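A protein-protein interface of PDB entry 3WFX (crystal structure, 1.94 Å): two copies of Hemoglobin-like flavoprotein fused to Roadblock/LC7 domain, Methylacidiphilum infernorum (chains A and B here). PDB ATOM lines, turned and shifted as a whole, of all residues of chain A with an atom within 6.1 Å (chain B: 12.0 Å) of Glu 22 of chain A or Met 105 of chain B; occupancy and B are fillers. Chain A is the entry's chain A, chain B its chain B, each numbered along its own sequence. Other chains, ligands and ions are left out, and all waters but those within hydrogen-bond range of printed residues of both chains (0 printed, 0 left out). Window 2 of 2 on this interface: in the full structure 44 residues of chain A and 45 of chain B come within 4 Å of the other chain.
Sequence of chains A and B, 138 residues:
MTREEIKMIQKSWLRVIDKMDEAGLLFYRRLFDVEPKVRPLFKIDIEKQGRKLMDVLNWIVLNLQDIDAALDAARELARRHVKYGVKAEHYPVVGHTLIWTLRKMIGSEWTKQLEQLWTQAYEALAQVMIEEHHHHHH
O of Met 105 of chain B is in hydrogen-bond range of NZ of Lys 19 of chain A, at 3.3 Å.
The side-chain hydroxyl (OG1) of Thr 101 of chain B sits at hydrogen-bond distance from the backbone carbonyl oxygen (O) of Thr 97 of chain B.
Val 16 of chain A touches Leu 102 of chain B. Val 16 of chain A touches Ile 106 of chain B (CG2 to CG1, 3.9 Å). Met 105 of chain B touches Glu 22 of chain A (CE to CG, 3.7 Å). CG2 of Thr 101 of chain B touches O of Ala 23 of chain A, 3.4 Å away. Met 105 of chain B touches Ala 23 of chain A (CE to N, 3.6 Å). Leu 26 of chain A touches Trp 100 of chain B (CG to CZ3, 3.5 Å). CB of Lys 104 of chain B touches CD2 of Leu 26 of chain A (3.6 Å). Leu 26 of chain A touches Met 105 of chain B. O of Phe 27 of chain A touches CG2 of Thr 97 of chain B (3.6 Å). OG1 of Thr 101 of chain B touches CA of Phe 27 of chain A (3.4 Å).
Of the printed residues of chain B, Val 16 of chain A touches Leu 102 (3.7 Å) and Ile 106 (3.9 Å). Asp 21 of chain A touches none of the printed residues of chain B. Printed residues of chain B within 4 Å of Glu 22 of chain A: Met 105. No residue of chain B comes within 4 Å of Leu 25 of chain A. Of the printed residues of chain A, Thr 97 of chain B touches Phe 27. Of the printed residues of chain A, Thr 101 of chain B touches Ala 23 (3.4 Å) and Phe 27 (3.4 Å). Printed residues of chain A within 4 Å of Lys 104 of chain B: Leu 26. Of the printed residues of chain A, Met 105 of chain B touches Lys 19 (3.3 Å), Glu 22 (3.7 Å), Ala 23 (3.6 Å) and Leu 26 (3.98 Å). Trp 110 of chain B touches none of the printed residues of chain A. Thr 111 of chain B touches none of the printed residues of chain A. The nearest printed residue of chain B that does not touch Glu 22 of chain A is Thr 101 of chain B (5.8 Å). The nearest printed residue of chain B that does not touch Leu 26 of chain A is Thr 101 of chain B (4.2 Å).
Printed residues of chain A that touch a printed residue of chain B: Val 16, Lys 19, Glu 22, Ala 23, Leu 26 and Phe 27. Hydrophobic or aromatic side chains of chain A within 4 Å of the printed part of chain B: Val 16, Ala 23, Leu 26 and Phe 27. Printed residues of chain B that touch a printed residue of chain A: Thr 97, Leu 98, Trp 100, Thr 101, Leu 102, Lys 104, Met 105 and Ile 106. Hydrophobic or aromatic side chains of chain B within 4 Å of the printed part of chain A: Leu 98, Trp 100, Leu 102, Met 105 and Ile 106. Along chain B the printed residues that touch a printed residue of chain A span positions 97 to 106. Among the printed residues, no Asp or Glu carboxylate lies within 4 Å of a Lys or Arg side-chain nitrogen of the other chain.
No position is printed for both chains.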
ATOM      1  N   VAL A  16      -8.355  32.222   7.090  1.00  0.00           N
ATOM      2  CA  VAL A  16      -8.390  30.782   6.823  1.00  0.00           C
ATOM      3  C   VAL A  16      -7.394  30.362   5.738  1.00  0.00           C
ATOM      4  O   VAL A  16      -6.857  29.256   5.759  1.00  0.00           O
ATOM      5  CB  VAL A  16      -9.821  30.333   6.436  1.00  0.00           C
ATOM      6  CG1 VAL A  16      -9.834  28.889   5.913  1.00  0.00           C
ATOM      7  CG2 VAL A  16     -10.744  30.484   7.628  1.00  0.00           C
ATOM      8  N   LYS A  19      -4.316  28.808   7.016  1.00  0.00           N
ATOM      9  CA  LYS A  19      -4.357  27.418   7.473  1.00  0.00           C
ATOM     10  C   LYS A  19      -5.152  26.529   6.516  1.00  0.00           C
ATOM     11  O   LYS A  19      -5.990  25.730   6.936  1.00  0.00           O
ATOM     12  CB  LYS A  19      -4.953  27.339   8.883  1.00  0.00           C
ATOM     13  CG  LYS A  19      -4.168  28.090   9.955  1.00  0.00           C
ATOM     14  CD  LYS A  19      -4.682  27.764  11.357  1.00  0.00           C
ATOM     15  CE  LYS A  19      -6.120  28.218  11.551  1.00  0.00           C
ATOM     16  NZ  LYS A  19      -6.705  27.721  12.835  1.00  0.00           N
ATOM     17  N   MET A  20      -4.877  26.651   5.224  1.00  0.00           N
ATOM     18  CA  MET A  20      -5.709  26.005   4.216  1.00  0.00           C
ATOM     19  C   MET A  20      -5.736  24.469   4.197  1.00  0.00           C
ATOM     20  O   MET A  20      -6.785  23.877   3.958  1.00  0.00           O
ATOM     21  CB  MET A  20      -5.383  26.547   2.819  1.00  0.00           C
ATOM     22  CG  MET A  20      -3.906  26.682   2.489  1.00  0.00           C
ATOM     23  SD  MET A  20      -3.679  27.484   0.879  1.00  0.00           S
ATOM     24  CE  MET A  20      -4.413  26.269  -0.215  1.00  0.00           C
ATOM     25  N   ASP A  21      -4.593  23.821   4.422  1.00  0.00           N
ATOM     26  CA  ASP A  21      -4.581  22.365   4.503  1.00  0.00           C
ATOM     27  C   ASP A  21      -5.447  21.876   5.650  1.00  0.00           C
ATOM     28  O   ASP A  21      -6.214  20.929   5.491  1.00  0.00           O
ATOM     29  CB  ASP A  21      -3.151  21.823   4.675  1.00  0.00           C
ATOM     30  CG  ASP A  21      -2.359  21.853   3.379  1.00  0.00           C
ATOM     31  OD1 ASP A  21      -2.993  21.933   2.300  1.00  0.00           O
ATOM     32  OD2 ASP A  21      -1.109  21.779   3.442  1.00  0.00           O
ATOM     33  N   GLU A  22      -5.321  22.515   6.808  1.00  0.00           N
ATOM     34  CA  GLU A  22      -6.144  22.136   7.948  1.00  0.00           C
ATOM     35  C   GLU A  22      -7.631  22.351   7.672  1.00  0.00           C
ATOM     36  O   GLU A  22      -8.472  21.503   8.012  1.00  0.00           O
ATOM     37  CB  GLU A  22      -5.730  22.895   9.211  1.00  0.00           C
ATOM     38  CG  GLU A  22      -6.530  22.453  10.430  1.00  0.00           C
ATOM     39  CD  GLU A  22      -6.156  23.188  11.700  1.00  0.00           C
ATOM     40  OE1 GLU A  22      -5.212  24.006  11.658  1.00  0.00           O
ATOM     41  OE2 GLU A  22      -6.811  22.943  12.742  1.00  0.00           O
ATOM     42  N   ALA A  23      -7.962  23.491   7.074  1.00  0.00           N
ATOM     43  CA  ALA A  23      -9.356  23.803   6.773  1.00  0.00           C
ATOM     44  C   ALA A  23      -9.921  22.778   5.795  1.00  0.00           C
ATOM     45  O   ALA A  23     -11.048  22.306   5.947  1.00  0.00           O
ATOM     46  CB  ALA A  23      -9.481  25.217   6.218  1.00  0.00           C
ATOM     47  N   GLY A  24      -9.115  22.428   4.795  1.00  0.00           N
ATOM     48  CA  GLY A  24      -9.520  21.476   3.784  1.00  0.00           C
ATOM     49  C   GLY A  24      -9.846  20.141   4.392  1.00  0.00           C
ATOM     50  O   GLY A  24     -10.901  19.581   4.108  1.00  0.00           O
ATOM     51  N   LEU A  25      -8.943  19.622   5.232  1.00  0.00           N
ATOM     52  CA  LEU A  25      -9.164  18.325   5.858  1.00  0.00           C
ATOM     53  C   LEU A  25     -10.434  18.326   6.702  1.00  0.00           C
ATOM     54  O   LEU A  25     -11.218  17.369   6.678  1.00  0.00           O
ATOM     55  CB  LEU A  25      -7.960  17.913   6.718  1.00  0.00           C
ATOM     56  CG  LEU A  25      -6.654  17.695   5.956  1.00  0.00           C
ATOM     57  CD1 LEU A  25      -5.481  17.438   6.935  1.00  0.00           C
ATOM     58  CD2 LEU A  25      -6.818  16.536   4.991  1.00  0.00           C
ATOM     59  N   LEU A  26     -10.628  19.404   7.450  1.00  0.00           N
ATOM     60  CA  LEU A  26     -11.802  19.560   8.291  1.00  0.00           C
ATOM     61  C   LEU A  26     -13.094  19.557   7.480  1.00  0.00           C
ATOM     62  O   LEU A  26     -14.067  18.913   7.866  1.00  0.00           O
ATOM     63  CB  LEU A  26     -11.703  20.853   9.099  1.00  0.00           C
ATOM     64  CG  LEU A  26     -12.713  21.034  10.220  1.00  0.00           C
ATOM     65  CD1 LEU A  26     -12.644  19.843  11.164  1.00  0.00           C
ATOM     66  CD2 LEU A  26     -12.423  22.322  10.978  1.00  0.00           C
ATOM     67  N   PHE A  27     -13.106  20.295   6.371  1.00  0.00           N
ATOM     68  CA  PHE A  27     -14.293  20.357   5.535  1.00  0.00           C
ATOM     69  C   PHE A  27     -14.733  18.964   5.055  1.00  0.00           C
ATOM     70  O   PHE A  27     -15.872  18.551   5.307  1.00  0.00           O
ATOM     71  CB  PHE A  27     -14.081  21.285   4.337  1.00  0.00           C
ATOM     72  CG  PHE A  27     -15.226  21.275   3.362  1.00  0.00           C
ATOM     73  CD1 PHE A  27     -16.349  22.046   3.596  1.00  0.00           C
ATOM     74  CD2 PHE A  27     -15.180  20.491   2.212  1.00  0.00           C
ATOM     75  CE1 PHE A  27     -17.413  22.036   2.711  1.00  0.00           C
ATOM     76  CE2 PHE A  27     -16.241  20.477   1.327  1.00  0.00           C
ATOM     77  CZ  PHE A  27     -17.353  21.260   1.579  1.00  0.00           C
ATOM     78  N   GLN A  49      -6.646  18.717  -1.428  1.00  0.00           N
ATOM     79  CA  GLN A  49      -7.893  19.004  -0.716  1.00  0.00           C
ATOM     80  C   GLN A  49      -7.927  20.424  -0.163  1.00  0.00           C
ATOM     81  O   GLN A  49      -8.964  21.075  -0.226  1.00  0.00           O
ATOM     82  CB  GLN A  49      -8.201  17.959   0.376  1.00  0.00           C
ATOM     83  CG  GLN A  49      -7.913  18.412   1.808  1.00  0.00           C
ATOM     84  CD  GLN A  49      -6.432  18.365   2.086  1.00  0.00           C
ATOM     85  OE1 GLN A  49      -5.937  18.958   3.045  1.00  0.00           O
ATOM     86  NE2 GLN A  49      -5.706  17.659   1.227  1.00  0.00           N
ATOM     87  N   HIS B  96     -23.822  24.508   5.107  1.00  0.00           N
ATOM     88  CA  HIS B  96     -23.678  24.347   6.550  1.00  0.00           C
ATOM     89  C   HIS B  96     -22.249  23.895   6.889  1.00  0.00           C
ATOM     90  O   HIS B  96     -21.648  24.336   7.867  1.00  0.00           O
ATOM     91  CB  HIS B  96     -24.679  23.303   7.045  1.00  0.00           C
ATOM     92  CG  HIS B  96     -24.739  23.180   8.536  1.00  0.00           C
ATOM     93  ND1 HIS B  96     -23.907  22.342   9.248  1.00  0.00           N
ATOM     94  CD2 HIS B  96     -25.541  23.784   9.448  1.00  0.00           C
ATOM     95  CE1 HIS B  96     -24.187  22.438  10.537  1.00  0.00           C
ATOM     96  NE2 HIS B  96     -25.179  23.303  10.684  1.00  0.00           N
ATOM     97  N   THR B  97     -21.712  23.014   6.059  1.00  0.00           N
ATOM     98  CA  THR B  97     -20.400  22.425   6.324  1.00  0.00           C
ATOM     99  C   THR B  97     -19.261  23.425   6.093  1.00  0.00           C
ATOM    100  O   THR B  97     -18.269  23.452   6.823  1.00  0.00           O
ATOM    101  CB  THR B  97     -20.191  21.150   5.492  1.00  0.00           C
ATOM    102  OG1 THR B  97     -21.238  20.227   5.785  1.00  0.00           O
ATOM    103  CG2 THR B  97     -18.818  20.486   5.841  1.00  0.00           C
ATOM    104  N   LEU B  98     -19.430  24.244   5.066  1.00  0.00           N
ATOM    105  CA  LEU B  98     -18.511  25.322   4.746  1.00  0.00           C
ATOM    106  C   LEU B  98     -18.430  26.341   5.889  1.00  0.00           C
ATOM    107  O   LEU B  98     -17.345  26.733   6.330  1.00  0.00           O
ATOM    108  CB  LEU B  98     -19.013  26.011   3.476  1.00  0.00           C
ATOM    109  CG  LEU B  98     -18.096  26.469   2.352  1.00  0.00           C
ATOM    110  CD1 LEU B  98     -16.985  25.472   2.112  1.00  0.00           C
ATOM    111  CD2 LEU B  98     -18.936  26.639   1.083  1.00  0.00           C
ATOM    112  N   ILE B  99     -19.583  26.773   6.363  1.00  0.00           N
ATOM    113  CA  ILE B  99     -19.623  27.760   7.437  1.00  0.00           C
ATOM    114  C   ILE B  99     -19.197  27.134   8.771  1.00  0.00           C
ATOM    115  O   ILE B  99     -18.544  27.784   9.582  1.00  0.00           O
ATOM    116  CB  ILE B  99     -21.011  28.425   7.521  1.00  0.00           C
ATOM    117  CG1 ILE B  99     -21.286  29.202   6.230  1.00  0.00           C
ATOM    118  CG2 ILE B  99     -21.090  29.385   8.709  1.00  0.00           C
ATOM    119  CD1 ILE B  99     -22.712  29.742   6.097  1.00  0.00           C
ATOM    120  N   TRP B 100     -19.526  25.862   8.972  1.00  0.00           N
ATOM    121  CA  TRP B 100     -19.029  25.114  10.136  1.00  0.00           C
ATOM    122  C   TRP B 100     -17.498  25.084  10.168  1.00  0.00           C
ATOM    123  O   TRP B 100     -16.867  25.279  11.216  1.00  0.00           O
ATOM    124  CB  TRP B 100     -19.591  23.692  10.115  1.00  0.00           C
ATOM    125  CG  TRP B 100     -19.280  22.861  11.329  1.00  0.00           C
ATOM    126  CD1 TRP B 100     -20.038  22.740  12.466  1.00  0.00           C
ATOM    127  CD2 TRP B 100     -18.142  22.018  11.514  1.00  0.00           C
ATOM    128  NE1 TRP B 100     -19.426  21.883  13.350  1.00  0.00           N
ATOM    129  CE2 TRP B 100     -18.263  21.421  12.788  1.00  0.00           C
ATOM    130  CE3 TRP B 100     -17.028  21.712  10.730  1.00  0.00           C
ATOM    131  CZ2 TRP B 100     -17.312  20.540  13.292  1.00  0.00           C
ATOM    132  CZ3 TRP B 100     -16.092  20.827  11.227  1.00  0.00           C
ATOM    133  CH2 TRP B 100     -16.235  20.255  12.497  1.00  0.00           C
ATOM    134  N   THR B 101     -16.900  24.848   9.006  1.00  0.00           N
ATOM    135  CA  THR B 101     -15.449  24.839   8.871  1.00  0.00           C
ATOM    136  C   THR B 101     -14.851  26.222   9.173  1.00  0.00           C
ATOM    137  O   THR B 101     -13.864  26.341   9.901  1.00  0.00           O
ATOM    138  CB  THR B 101     -15.035  24.331   7.471  1.00  0.00           C
ATOM    139  OG1 THR B 101     -15.553  23.008   7.278  1.00  0.00           O
ATOM    140  CG2 THR B 101     -13.509  24.290   7.325  1.00  0.00           C
ATOM    141  N   LEU B 102     -15.465  27.274   8.645  1.00  0.00           N
ATOM    142  CA  LEU B 102     -14.948  28.627   8.881  1.00  0.00           C
ATOM    143  C   LEU B 102     -15.034  28.947  10.373  1.00  0.00           C
ATOM    144  O   LEU B 102     -14.078  29.460  10.979  1.00  0.00           O
ATOM    145  CB  LEU B 102     -15.742  29.665   8.065  1.00  0.00           C
ATOM    146  CG  LEU B 102     -15.529  29.711   6.545  1.00  0.00           C
ATOM    147  CD1 LEU B 102     -16.603  30.601   5.880  1.00  0.00           C
ATOM    148  CD2 LEU B 102     -14.149  30.229   6.195  1.00  0.00           C
ATOM    149  N   ARG B 103     -16.178  28.631  10.968  1.00  0.00           N
ATOM    150  CA  ARG B 103     -16.357  28.840  12.407  1.00  0.00           C
ATOM    151  C   ARG B 103     -15.315  28.083  13.237  1.00  0.00           C
ATOM    152  O   ARG B 103     -14.701  28.663  14.128  1.00  0.00           O
ATOM    153  CB  ARG B 103     -17.771  28.460  12.858  1.00  0.00           C
ATOM    154  CG  ARG B 103     -17.964  28.508  14.374  1.00  0.00           C
ATOM    155  CD  ARG B 103     -19.434  28.401  14.748  1.00  0.00           C
ATOM    156  NE  ARG B 103     -20.024  27.119  14.373  1.00  0.00           N
ATOM    157  CZ  ARG B 103     -20.045  26.051  15.169  1.00  0.00           C
ATOM    158  NH1 ARG B 103     -19.500  26.108  16.377  1.00  0.00           N
ATOM    159  NH2 ARG B 103     -20.620  24.930  14.762  1.00  0.00           N
ATOM    160  N   LYS B 104     -15.094  26.803  12.935  1.00  0.00           N
ATOM    161  CA  LYS B 104     -14.098  26.037  13.675  1.00  0.00           C
ATOM    162  C   LYS B 104     -12.690  26.606  13.510  1.00  0.00           C
ATOM    163  O   LYS B 104     -11.934  26.702  14.487  1.00  0.00           O
ATOM    164  CB  LYS B 104     -14.123  24.556  13.279  1.00  0.00           C
ATOM    165  CG  LYS B 104     -15.363  23.807  13.737  1.00  0.00           C
ATOM    166  CD  LYS B 104     -15.506  23.789  15.263  1.00  0.00           C
ATOM    167  CE  LYS B 104     -16.853  23.156  15.649  1.00  0.00           C
ATOM    168  NZ  LYS B 104     -17.178  23.235  17.098  1.00  0.00           N
ATOM    169  N   MET B 105     -12.347  26.979  12.277  1.00  0.00           N
ATOM    170  CA  MET B 105     -11.010  27.489  11.984  1.00  0.00           C
ATOM    171  C   MET B 105     -10.763  28.865  12.609  1.00  0.00           C
ATOM    172  O   MET B 105      -9.692  29.107  13.174  1.00  0.00           O
ATOM    173  CB  MET B 105     -10.760  27.542  10.472  1.00  0.00           C
ATOM    174  CG  MET B 105     -10.800  26.181   9.784  1.00  0.00           C
ATOM    175  SD  MET B 105      -9.569  25.036  10.434  1.00  0.00           S
ATOM    176  CE  MET B 105      -8.074  25.800   9.807  1.00  0.00           C
ATOM    177  N   ILE B 106     -11.739  29.754  12.507  1.00  0.00           N
ATOM    178  CA  ILE B 106     -11.572  31.121  13.010  1.00  0.00           C
ATOM    179  C   ILE B 106     -11.632  31.193  14.547  1.00  0.00           C
ATOM    180  O   ILE B 106     -11.067  32.098  15.161  1.00  0.00           O
ATOM    181  CB  ILE B 106     -12.538  32.105  12.293  1.00  0.00           C
ATOM    182  CG1 ILE B 106     -12.105  32.264  10.831  1.00  0.00           C
ATOM    183  CG2 ILE B 106     -12.567  33.471  12.981  1.00  0.00           C
ATOM    184  CD1 ILE B 106     -13.220  32.664   9.900  1.00  0.00           C
ATOM    185  N   GLY B 107     -12.302  30.222  15.159  1.00  0.00           N
ATOM    186  CA  GLY B 107     -12.263  30.057  16.602  1.00  0.00           C
ATOM    187  C   GLY B 107     -12.894  31.190  17.395  1.00  0.00           C
ATOM    188  O   GLY B 107     -14.046  31.557  17.164  1.00  0.00           O
ATOM    189  N   SER B 108     -12.125  31.748  18.326  1.00  0.00           N
ATOM    190  CA  SER B 108     -12.642  32.734  19.275  1.00  0.00           C
ATOM    191  C   SER B 108     -13.000  34.059  18.625  1.00  0.00           C
ATOM    192  O   SER B 108     -13.789  34.832  19.171  1.00  0.00           O
ATOM    193  CB  SER B 108     -11.633  32.965  20.401  1.00  0.00           C
ATOM    194  OG  SER B 108     -10.318  33.069  19.883  1.00  0.00           O
ATOM    195  N   GLU B 109     -12.418  34.323  17.459  1.00  0.00           N
ATOM    196  CA  GLU B 109     -12.696  35.558  16.738  1.00  0.00           C
ATOM    197  C   GLU B 109     -13.954  35.470  15.870  1.00  0.00           C
ATOM    198  O   GLU B 109     -14.276  36.410  15.148  1.00  0.00           O
ATOM    199  CB  GLU B 109     -11.503  35.964  15.879  1.00  0.00           C
ATOM    200  CG  GLU B 109     -10.268  36.348  16.665  1.00  0.00           C
ATOM    201  CD  GLU B 109      -9.179  35.301  16.574  1.00  0.00           C
ATOM    202  OE1 GLU B 109      -9.508  34.097  16.564  1.00  0.00           O
ATOM    203  OE2 GLU B 109      -7.993  35.686  16.494  1.00  0.00           O
ATOM    204  N   TRP B 110     -14.662  34.345  15.930  1.00  0.00           N
ATOM    205  CA  TRP B 110     -15.890  34.196  15.146  1.00  0.00           C
ATOM    206  C   TRP B 110     -17.012  34.950  15.847  1.00  0.00           C
ATOM    207  O   TRP B 110     -17.012  35.076  17.070  1.00  0.00           O
ATOM    208  CB  TRP B 110     -16.242  32.714  15.002  1.00  0.00           C
ATOM    209  CG  TRP B 110     -17.395  32.383  14.081  1.00  0.00           C
ATOM    210  CD1 TRP B 110     -18.636  31.973  14.456  1.00  0.00           C
ATOM    211  CD2 TRP B 110     -17.396  32.402  12.643  1.00  0.00           C
ATOM    212  NE1 TRP B 110     -19.414  31.735  13.350  1.00  0.00           N
ATOM    213  CE2 TRP B 110     -18.681  31.996  12.224  1.00  0.00           C
ATOM    214  CE3 TRP B 110     -16.442  32.729  11.673  1.00  0.00           C
ATOM    215  CZ2 TRP B 110     -19.038  31.898  10.877  1.00  0.00           C
ATOM    216  CZ3 TRP B 110     -16.793  32.636  10.327  1.00  0.00           C
ATOM    217  CH2 TRP B 110     -18.087  32.221   9.942  1.00  0.00           C
ATOM    218  N   THR B 111     -17.957  35.466  15.073  1.00  0.00           N
ATOM    219  CA  THR B 111     -19.082  36.213  15.630  1.00  0.00           C
ATOM    220  C   THR B 111     -20.374  35.801  14.939  1.00  0.00           C
ATOM    221  O   THR B 111     -20.348  35.226  13.849  1.00  0.00           O
ATOM    222  CB  THR B 111     -18.914  37.739  15.438  1.00  0.00           C
ATOM    223  OG1 THR B 111     -18.919  38.066  14.038  1.00  0.00           O
ATOM    224  CG2 THR B 111     -17.628  38.237  16.078  1.00  0.00           C
ATOM    225  N   LEU B 114     -20.494  37.607  11.547  1.00  0.00           N
ATOM    226  CA  LEU B 114     -19.764  36.922  10.489  1.00  0.00           C
ATOM    227  C   LEU B 114     -20.549  35.728   9.977  1.00  0.00           C
ATOM    228  O   LEU B 114     -20.628  35.504   8.773  1.00  0.00           O
ATOM    229  CB  LEU B 114     -18.407  36.443  10.984  1.00  0.00           C
ATOM    230  CG  LEU B 114     -17.197  37.315  10.679  1.00  0.00           C
ATOM    231  CD1 LEU B 114     -15.984  36.660  11.304  1.00  0.00           C
ATOM    232  CD2 LEU B 114     -17.015  37.491   9.168  1.00  0.00           C
ATOM    233  N   GLU B 115     -21.118  34.956  10.895  1.00  0.00           N
ATOM    234  CA  GLU B 115     -21.887  33.783  10.509  1.00  0.00           C
ATOM    235  C   GLU B 115     -23.124  34.151   9.698  1.00  0.00           C
ATOM    236  O   GLU B 115     -23.492  33.454   8.746  1.00  0.00           O
ATOM    237  CB  GLU B 115     -22.263  32.956  11.738  1.00  0.00           C
ATOM    238  CG  GLU B 115     -22.974  31.673  11.407  1.00  0.00           C
ATOM    239  CD  GLU B 115     -22.821  30.641  12.498  1.00  0.00           C
ATOM    240  OE1 GLU B 115     -21.974  30.844  13.392  1.00  0.00           O
ATOM    241  OE2 GLU B 115     -23.550  29.627  12.461  1.00  0.00           O
ATOM    242  N   TRP B 118     -21.729  35.251   6.006  1.00  0.00           N
ATOM    243  CA  TRP B 118     -21.414  34.099   5.165  1.00  0.00           C
ATOM    244  C   TRP B 118     -22.683  33.340   4.780  1.00  0.00           C
ATOM    245  O   TRP B 118     -22.819  32.889   3.643  1.00  0.00           O
ATOM    246  CB  TRP B 118     -20.410  33.160   5.851  1.00  0.00           C
ATOM    247  CG  TRP B 118     -18.955  33.610   5.721  1.00  0.00           C
ATOM    248  CD1 TRP B 118     -18.216  34.249   6.670  1.00  0.00           C
ATOM    249  CD2 TRP B 118     -18.081  33.423   4.591  1.00  0.00           C
ATOM    250  NE1 TRP B 118     -16.940  34.481   6.207  1.00  0.00           N
ATOM    251  CE2 TRP B 118     -16.830  33.984   4.933  1.00  0.00           C
ATOM    252  CE3 TRP B 118     -18.237  32.838   3.325  1.00  0.00           C
ATOM    253  CZ2 TRP B 118     -15.735  33.977   4.056  1.00  0.00           C
ATOM    254  CZ3 TRP B 118     -17.150  32.838   2.446  1.00  0.00           C
ATOM    255  CH2 TRP B 118     -15.908  33.394   2.823  1.00  0.00           C
